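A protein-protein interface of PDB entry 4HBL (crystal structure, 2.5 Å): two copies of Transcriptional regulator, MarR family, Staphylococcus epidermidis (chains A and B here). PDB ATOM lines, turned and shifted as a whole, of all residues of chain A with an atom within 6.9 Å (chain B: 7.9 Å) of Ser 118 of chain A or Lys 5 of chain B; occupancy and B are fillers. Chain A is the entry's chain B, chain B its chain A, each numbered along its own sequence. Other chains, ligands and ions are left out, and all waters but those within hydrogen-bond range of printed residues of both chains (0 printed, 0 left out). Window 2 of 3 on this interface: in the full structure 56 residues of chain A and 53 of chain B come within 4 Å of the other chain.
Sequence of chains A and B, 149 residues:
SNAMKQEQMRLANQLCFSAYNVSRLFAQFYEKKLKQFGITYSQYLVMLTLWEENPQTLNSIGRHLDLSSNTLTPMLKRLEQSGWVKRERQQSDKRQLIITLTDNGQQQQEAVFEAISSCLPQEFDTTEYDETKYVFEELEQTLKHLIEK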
ATOM      1  N   LYS A  33      15.501 -34.021  21.412  1.00  0.00           N
ATOM      2  CA  LYS A  33      14.134 -33.581  21.136  1.00  0.00           C
ATOM      3  C   LYS A  33      13.616 -33.814  19.662  1.00  0.00           C
ATOM      4  O   LYS A  33      12.427 -33.730  19.391  1.00  0.00           O
ATOM      5  CB  LYS A  33      13.960 -32.125  21.598  1.00  0.00           C
ATOM      6  CG  LYS A  33      14.396 -31.844  23.036  1.00  0.00           C
ATOM      7  CD  LYS A  33      13.567 -32.609  24.086  1.00  0.00           C
ATOM      8  CE  LYS A  33      12.181 -31.994  24.293  1.00  0.00           C
ATOM      9  NZ  LYS A  33      11.441 -32.619  25.417  1.00  0.00           N
ATOM     10  N   PHE A 113       9.388 -26.515  17.183  1.00  0.00           N
ATOM     11  CA  PHE A 113       9.979 -25.386  17.933  1.00  0.00           C
ATOM     12  C   PHE A 113       9.555 -25.407  19.375  1.00  0.00           C
ATOM     13  O   PHE A 113      10.330 -25.079  20.271  1.00  0.00           O
ATOM     14  CB  PHE A 113       9.618 -24.038  17.315  1.00  0.00           C
ATOM     15  CG  PHE A 113      10.493 -23.658  16.151  1.00  0.00           C
ATOM     16  CD1 PHE A 113      11.320 -24.589  15.540  1.00  0.00           C
ATOM     17  CD2 PHE A 113      10.494 -22.365  15.671  1.00  0.00           C
ATOM     18  CE1 PHE A 113      12.133 -24.228  14.478  1.00  0.00           C
ATOM     19  CE2 PHE A 113      11.295 -21.994  14.610  1.00  0.00           C
ATOM     20  CZ  PHE A 113      12.098 -22.930  14.001  1.00  0.00           C
ATOM     21  N   GLU A 114       8.311 -25.802  19.586  1.00  0.00           N
ATOM     22  CA  GLU A 114       7.834 -26.043  20.913  1.00  0.00           C
ATOM     23  C   GLU A 114       8.762 -26.961  21.667  1.00  0.00           C
ATOM     24  O   GLU A 114       9.118 -26.674  22.810  1.00  0.00           O
ATOM     25  CB  GLU A 114       6.456 -26.686  20.873  1.00  0.00           C
ATOM     26  CG  GLU A 114       5.363 -25.746  21.303  1.00  0.00           C
ATOM     27  CD  GLU A 114       5.759 -25.007  22.573  1.00  0.00           C
ATOM     28  OE1 GLU A 114       6.149 -25.668  23.576  1.00  0.00           O
ATOM     29  OE2 GLU A 114       5.710 -23.761  22.560  1.00  0.00           O
ATOM     30  N   ALA A 115       9.166 -28.077  21.052  1.00  0.00           N
ATOM     31  CA  ALA A 115       9.787 -29.076  21.890  1.00  0.00           C
ATOM     32  C   ALA A 115      11.193 -28.632  22.227  1.00  0.00           C
ATOM     33  O   ALA A 115      11.721 -28.971  23.299  1.00  0.00           O
ATOM     34  CB  ALA A 115       9.750 -30.443  21.264  1.00  0.00           C
ATOM     35  N   ILE A 116      11.780 -27.845  21.317  1.00  0.00           N
ATOM     36  CA  ILE A 116      13.123 -27.371  21.535  1.00  0.00           C
ATOM     37  C   ILE A 116      13.168 -26.217  22.516  1.00  0.00           C
ATOM     38  O   ILE A 116      14.010 -26.231  23.414  1.00  0.00           O
ATOM     39  CB  ILE A 116      13.825 -27.001  20.218  1.00  0.00           C
ATOM     40  CG1 ILE A 116      13.982 -28.256  19.334  1.00  0.00           C
ATOM     41  CG2 ILE A 116      15.203 -26.382  20.474  1.00  0.00           C
ATOM     42  CD1 ILE A 116      14.196 -27.937  17.872  1.00  0.00           C
ATOM     43  N   SER A 117      12.280 -25.229  22.361  1.00  0.00           N
ATOM     44  CA  SER A 117      12.393 -23.999  23.159  1.00  0.00           C
ATOM     45  C   SER A 117      12.011 -24.199  24.606  1.00  0.00           C
ATOM     46  O   SER A 117      12.245 -23.327  25.419  1.00  0.00           O
ATOM     47  CB  SER A 117      11.624 -22.808  22.561  1.00  0.00           C
ATOM     48  OG  SER A 117      10.280 -23.132  22.375  1.00  0.00           O
ATOM     49  N   SER A 118      11.436 -25.348  24.930  1.00  0.00           N
ATOM     50  CA  SER A 118      11.199 -25.698  26.330  1.00  0.00           C
ATOM     51  C   SER A 118      12.485 -26.148  27.049  1.00  0.00           C
ATOM     52  O   SER A 118      12.542 -26.154  28.283  1.00  0.00           O
ATOM     53  CB  SER A 118      10.121 -26.782  26.438  1.00  0.00           C
ATOM     54  OG  SER A 118      10.528 -27.985  25.788  1.00  0.00           O
ATOM     55  N   CYS A 119      13.512 -26.525  26.283  1.00  0.00           N
ATOM     56  CA  CYS A 119      14.742 -27.065  26.849  1.00  0.00           C
ATOM     57  C   CYS A 119      15.844 -26.022  26.910  1.00  0.00           C
ATOM     58  O   CYS A 119      16.917 -26.221  27.491  1.00  0.00           O
ATOM     59  CB  CYS A 119      15.192 -28.248  26.010  1.00  0.00           C
ATOM     60  SG  CYS A 119      14.113 -29.668  26.226  1.00  0.00           S
ATOM     61  N   LEU A 120      15.560 -24.898  26.280  1.00  0.00           N
ATOM     62  CA  LEU A 120      16.473 -23.780  26.263  1.00  0.00           C
ATOM     63  C   LEU A 120      16.717 -23.244  27.680  1.00  0.00           C
ATOM     64  O   LEU A 120      15.896 -23.473  28.560  1.00  0.00           O
ATOM     65  CB  LEU A 120      15.940 -22.702  25.320  1.00  0.00           C
ATOM     66  CG  LEU A 120      16.159 -23.127  23.865  1.00  0.00           C
ATOM     67  CD1 LEU A 120      15.938 -21.959  22.921  1.00  0.00           C
ATOM     68  CD2 LEU A 120      17.547 -23.697  23.643  1.00  0.00           C
ATOM     69  N   PRO A 121      17.866 -22.572  27.913  1.00  0.00           N
ATOM     70  CA  PRO A 121      18.053 -21.988  29.235  1.00  0.00           C
ATOM     71  C   PRO A 121      17.085 -20.828  29.445  1.00  0.00           C
ATOM     72  O   PRO A 121      16.907 -20.004  28.541  1.00  0.00           O
ATOM     73  CB  PRO A 121      19.508 -21.482  29.202  1.00  0.00           C
ATOM     74  CG  PRO A 121      19.855 -21.338  27.750  1.00  0.00           C
ATOM     75  CD  PRO A 121      19.078 -22.433  27.074  1.00  0.00           C
ATOM     76  N   PHE A 124      18.942 -16.091  29.203  1.00  0.00           N
ATOM     77  CA  PHE A 124      19.507 -15.698  27.907  1.00  0.00           C
ATOM     78  C   PHE A 124      19.445 -14.173  27.714  1.00  0.00           C
ATOM     79  O   PHE A 124      18.642 -13.498  28.366  1.00  0.00           O
ATOM     80  CB  PHE A 124      18.800 -16.429  26.749  1.00  0.00           C
ATOM     81  CG  PHE A 124      17.712 -15.620  26.087  1.00  0.00           C
ATOM     82  CD1 PHE A 124      17.963 -14.939  24.895  1.00  0.00           C
ATOM     83  CD2 PHE A 124      16.445 -15.537  26.656  1.00  0.00           C
ATOM     84  CE1 PHE A 124      16.975 -14.190  24.289  1.00  0.00           C
ATOM     85  CE2 PHE A 124      15.451 -14.792  26.048  1.00  0.00           C
ATOM     86  CZ  PHE A 124      15.715 -14.119  24.864  1.00  0.00           C
ATOM     87  N   ASN B   2       6.851 -16.988  26.003  1.00  0.00           N
ATOM     88  CA  ASN B   2       5.882 -16.312  25.075  1.00  0.00           C
ATOM     89  C   ASN B   2       6.525 -15.785  23.778  1.00  0.00           C
ATOM     90  O   ASN B   2       6.570 -16.508  22.781  1.00  0.00           O
ATOM     91  CB  ASN B   2       5.074 -15.202  25.797  1.00  0.00           C
ATOM     92  CG  ASN B   2       3.843 -15.741  26.550  1.00  0.00           C
ATOM     93  OD1 ASN B   2       3.875 -16.832  27.137  1.00  0.00           O
ATOM     94  ND2 ASN B   2       2.754 -14.960  26.548  1.00  0.00           N
ATOM     95  N   ALA B   3       7.012 -14.541  23.787  1.00  0.00           N
ATOM     96  CA  ALA B   3       7.575 -13.919  22.575  1.00  0.00           C
ATOM     97  C   ALA B   3       9.098 -13.817  22.608  1.00  0.00           C
ATOM     98  O   ALA B   3       9.744 -13.908  21.573  1.00  0.00           O
ATOM     99  CB  ALA B   3       6.960 -12.545  22.324  1.00  0.00           C
ATOM    100  N   MET B   4       9.654 -13.608  23.798  1.00  0.00           N
ATOM    101  CA  MET B   4      11.098 -13.539  24.001  1.00  0.00           C
ATOM    102  C   MET B   4      11.689 -14.927  23.947  1.00  0.00           C
ATOM    103  O   MET B   4      12.849 -15.111  23.576  1.00  0.00           O
ATOM    104  CB  MET B   4      11.327 -12.897  25.367  1.00  0.00           C
ATOM    105  CG  MET B   4      12.738 -12.326  25.519  1.00  0.00           C
ATOM    106  SD  MET B   4      13.000 -10.666  24.473  1.00  0.00           S
ATOM    107  CE  MET B   4      14.887 -10.808  23.915  1.00  0.00           C
ATOM    108  N   LYS B   5      10.879 -15.906  24.337  1.00  0.00           N
ATOM    109  CA  LYS B   5      11.180 -17.327  24.222  1.00  0.00           C
ATOM    110  C   LYS B   5      11.263 -17.750  22.747  1.00  0.00           C
ATOM    111  O   LYS B   5      12.074 -18.604  22.382  1.00  0.00           O
ATOM    112  CB  LYS B   5      10.072 -18.101  24.930  1.00  0.00           C
ATOM    113  CG  LYS B   5      10.369 -19.531  25.335  1.00  0.00           C
ATOM    114  CD  LYS B   5       9.133 -20.092  26.040  1.00  0.00           C
ATOM    115  CE  LYS B   5       9.182 -21.604  26.163  1.00  0.00           C
ATOM    116  NZ  LYS B   5      10.400 -22.055  26.892  1.00  0.00           N
ATOM    117  N   GLN B   6      10.418 -17.148  21.910  1.00  0.00           N
ATOM    118  CA  GLN B   6      10.494 -17.303  20.465  1.00  0.00           C
ATOM    119  C   GLN B   6      11.765 -16.703  19.870  1.00  0.00           C
ATOM    120  O   GLN B   6      12.349 -17.267  18.948  1.00  0.00           O
ATOM    121  CB  GLN B   6       9.305 -16.648  19.791  1.00  0.00           C
ATOM    122  CG  GLN B   6       8.046 -17.487  19.796  1.00  0.00           C
ATOM    123  CD  GLN B   6       6.853 -16.746  19.213  1.00  0.00           C
ATOM    124  OE1 GLN B   6       6.219 -17.230  18.273  1.00  0.00           O
ATOM    125  NE2 GLN B   6       6.538 -15.567  19.769  1.00  0.00           N
ATOM    126  N   GLU B   7      12.176 -15.543  20.379  1.00  0.00           N
ATOM    127  CA  GLU B   7      13.411 -14.909  19.945  1.00  0.00           C
ATOM    128  C   GLU B   7      14.605 -15.781  20.203  1.00  0.00           C
ATOM    129  O   GLU B   7      15.470 -15.922  19.327  1.00  0.00           O
ATOM    130  CB  GLU B   7      13.593 -13.562  20.628  1.00  0.00           C
ATOM    131  CG  GLU B   7      13.124 -12.414  19.762  1.00  0.00           C
ATOM    132  CD  GLU B   7      13.784 -12.467  18.403  1.00  0.00           C
ATOM    133  OE1 GLU B   7      13.108 -12.813  17.408  1.00  0.00           O
ATOM    134  OE2 GLU B   7      14.998 -12.196  18.349  1.00  0.00           O
ATOM    135  N   GLN B   8      14.644 -16.370  21.400  1.00  0.00           N
ATOM    136  CA  GLN B   8      15.699 -17.309  21.796  1.00  0.00           C
ATOM    137  C   GLN B   8      15.858 -18.491  20.815  1.00  0.00           C
ATOM    138  O   GLN B   8      16.966 -18.914  20.521  1.00  0.00           O
ATOM    139  CB  GLN B   8      15.406 -17.845  23.184  1.00  0.00           C
ATOM    140  CG  GLN B   8      16.574 -18.573  23.815  1.00  0.00           C
ATOM    141  CD  GLN B   8      16.278 -19.006  25.227  1.00  0.00           C
ATOM    142  OE1 GLN B   8      15.141 -18.906  25.690  1.00  0.00           O
ATOM    143  NE2 GLN B   8      17.299 -19.474  25.930  1.00  0.00           N
ATOM    144  N   MET B   9      14.738 -18.998  20.318  1.00  0.00           N
ATOM    145  CA  MET B   9      14.704 -20.086  19.361  1.00  0.00           C
ATOM    146  C   MET B   9      15.240 -19.645  18.044  1.00  0.00           C
ATOM    147  O   MET B   9      15.980 -20.383  17.402  1.00  0.00           O
ATOM    148  CB  MET B   9      13.256 -20.447  19.063  1.00  0.00           C
ATOM    149  CG  MET B   9      12.860 -21.859  19.449  1.00  0.00           C
ATOM    150  SD  MET B   9      14.180 -23.223  18.996  1.00  0.00           S
ATOM    151  CE  MET B   9      12.891 -24.653  18.753  1.00  0.00           C
ATOM    152  N   ARG B  10      14.856 -18.461  17.605  1.00  0.00           N
ATOM    153  CA  ARG B  10      15.375 -17.930  16.340  1.00  0.00           C
ATOM    154  C   ARG B  10      16.909 -17.757  16.412  1.00  0.00           C
ATOM    155  O   ARG B  10      17.639 -18.111  15.479  1.00  0.00           O
ATOM    156  CB  ARG B  10      14.704 -16.600  15.992  1.00  0.00           C
ATOM    157  CG  ARG B  10      14.500 -16.376  14.507  1.00  0.00           C
ATOM    158  CD  ARG B  10      14.157 -14.925  14.185  1.00  0.00           C
ATOM    159  NE  ARG B  10      15.364 -14.204  13.772  1.00  0.00           N
ATOM    160  CZ  ARG B  10      15.896 -13.163  14.413  1.00  0.00           C
ATOM    161  NH1 ARG B  10      15.305 -12.671  15.499  1.00  0.00           N
ATOM    162  NH2 ARG B  10      17.026 -12.608  13.959  1.00  0.00           N
ATOM    163  N   LEU B  11      17.393 -17.249  17.539  1.00  0.00           N
ATOM    164  CA  LEU B  11      18.821 -16.974  17.690  1.00  0.00           C
ATOM    165  C   LEU B  11      19.591 -18.293  17.853  1.00  0.00           C
ATOM    166  O   LEU B  11      20.606 -18.527  17.167  1.00  0.00           O
ATOM    167  CB  LEU B  11      19.081 -15.966  18.828  1.00  0.00           C
ATOM    168  CG  LEU B  11      18.720 -14.491  18.563  1.00  0.00           C
ATOM    169  CD1 LEU B  11      18.388 -13.697  19.835  1.00  0.00           C
ATOM    170  CD2 LEU B  11      19.787 -13.751  17.745  1.00  0.00           C
ATOM    171  N   ALA B  12      19.090 -19.180  18.712  1.00  0.00           N
ATOM    172  CA  ALA B  12      19.644 -20.526  18.761  1.00  0.00           C
ATOM    173  C   ALA B  12      19.726 -21.240  17.390  1.00  0.00           C
ATOM    174  O   ALA B  12      20.718 -21.922  17.140  1.00  0.00           O
ATOM    175  CB  ALA B  12      18.893 -21.391  19.745  1.00  0.00           C
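NZ of Lys 5 of chain B sits at hydrogen-bond distance from O of Ser 117 of chain A, 2.7 Å away. The side-chain amide nitrogen (NE2) of Gln 8 of chain B lies within hydrogen-bond range of the backbone carbonyl oxygen (O) of Pro 121 of chain A (2.7 Å).
O of Phe 113 of chain A lies within hydrogen-bond range of OG of Ser 117 of chain A (2.9 Å). O of Ala 115 of chain A is in hydrogen-bond range of OG of Ser 118 of chain A.
CE of Met 9 of chain B touches O of Phe 113 of chain A, 3.0 Å away. Met 9 of chain B touches Ile 116 of chain A (CE to CB, 2.9 Å). CB of Ser 117 of chain A touches CG of Met 9 of chain B, 3.5 Å away. CA of Ser 118 of chain A touches NZ of Lys 5 of chain B, 3.8 Å away. CB of Leu 120 of chain A touches NE2 of Gln 8 of chain B, 3.6 Å away. CZ of Phe 124 of chain A touches O of Met 4 of chain B, at 3.3 Å. Phe 124 of chain A touches Gln 8 of chain B.
Of the printed residues of chain B, Phe 113 of chain A touches Met 9 (3.0 Å). Ala 115 of chain A touches none of the printed residues of chain B. Ser 117 of chain A touches just these residues of chain B: Lys 5 and Met 9. Of the printed residues of chain B, Ser 118 of chain A touches Lys 5. Printed residues of chain B within 4 Å of Phe 124 of chain A: Met 4 and Gln 8. Printed residues of chain A within 4 Å of Met 4 of chain B: Phe 124 (3.3 Å). Of chain A, only Ser 117 (2.7 Å) and Ser 118 (3.8 Å) come within 4 Å of Lys 5 of chain B. The nearest residue of chain A that does not touch Lys 5 of chain B is Phe 124 of chain A (5.0 Å). The nearest printed residue of chain B that does not touch Phe 113 of chain A is Arg 10 of chain B (5.8 Å).
Printed residues of chain A that touch a printed residue of chain B: Phe 113, Ile 116, Ser 117, Ser 118, Leu 120, Pro 121 and Phe 124. Along chain A the printed residues that touch a printed residue of chain B span positions 113 to 124. Among the printed residues, no Asp or Glu carboxylate lies within 4 Å of a Lys or Arg side-chain nitrogen of the other chain.
No position is printed for both chains.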
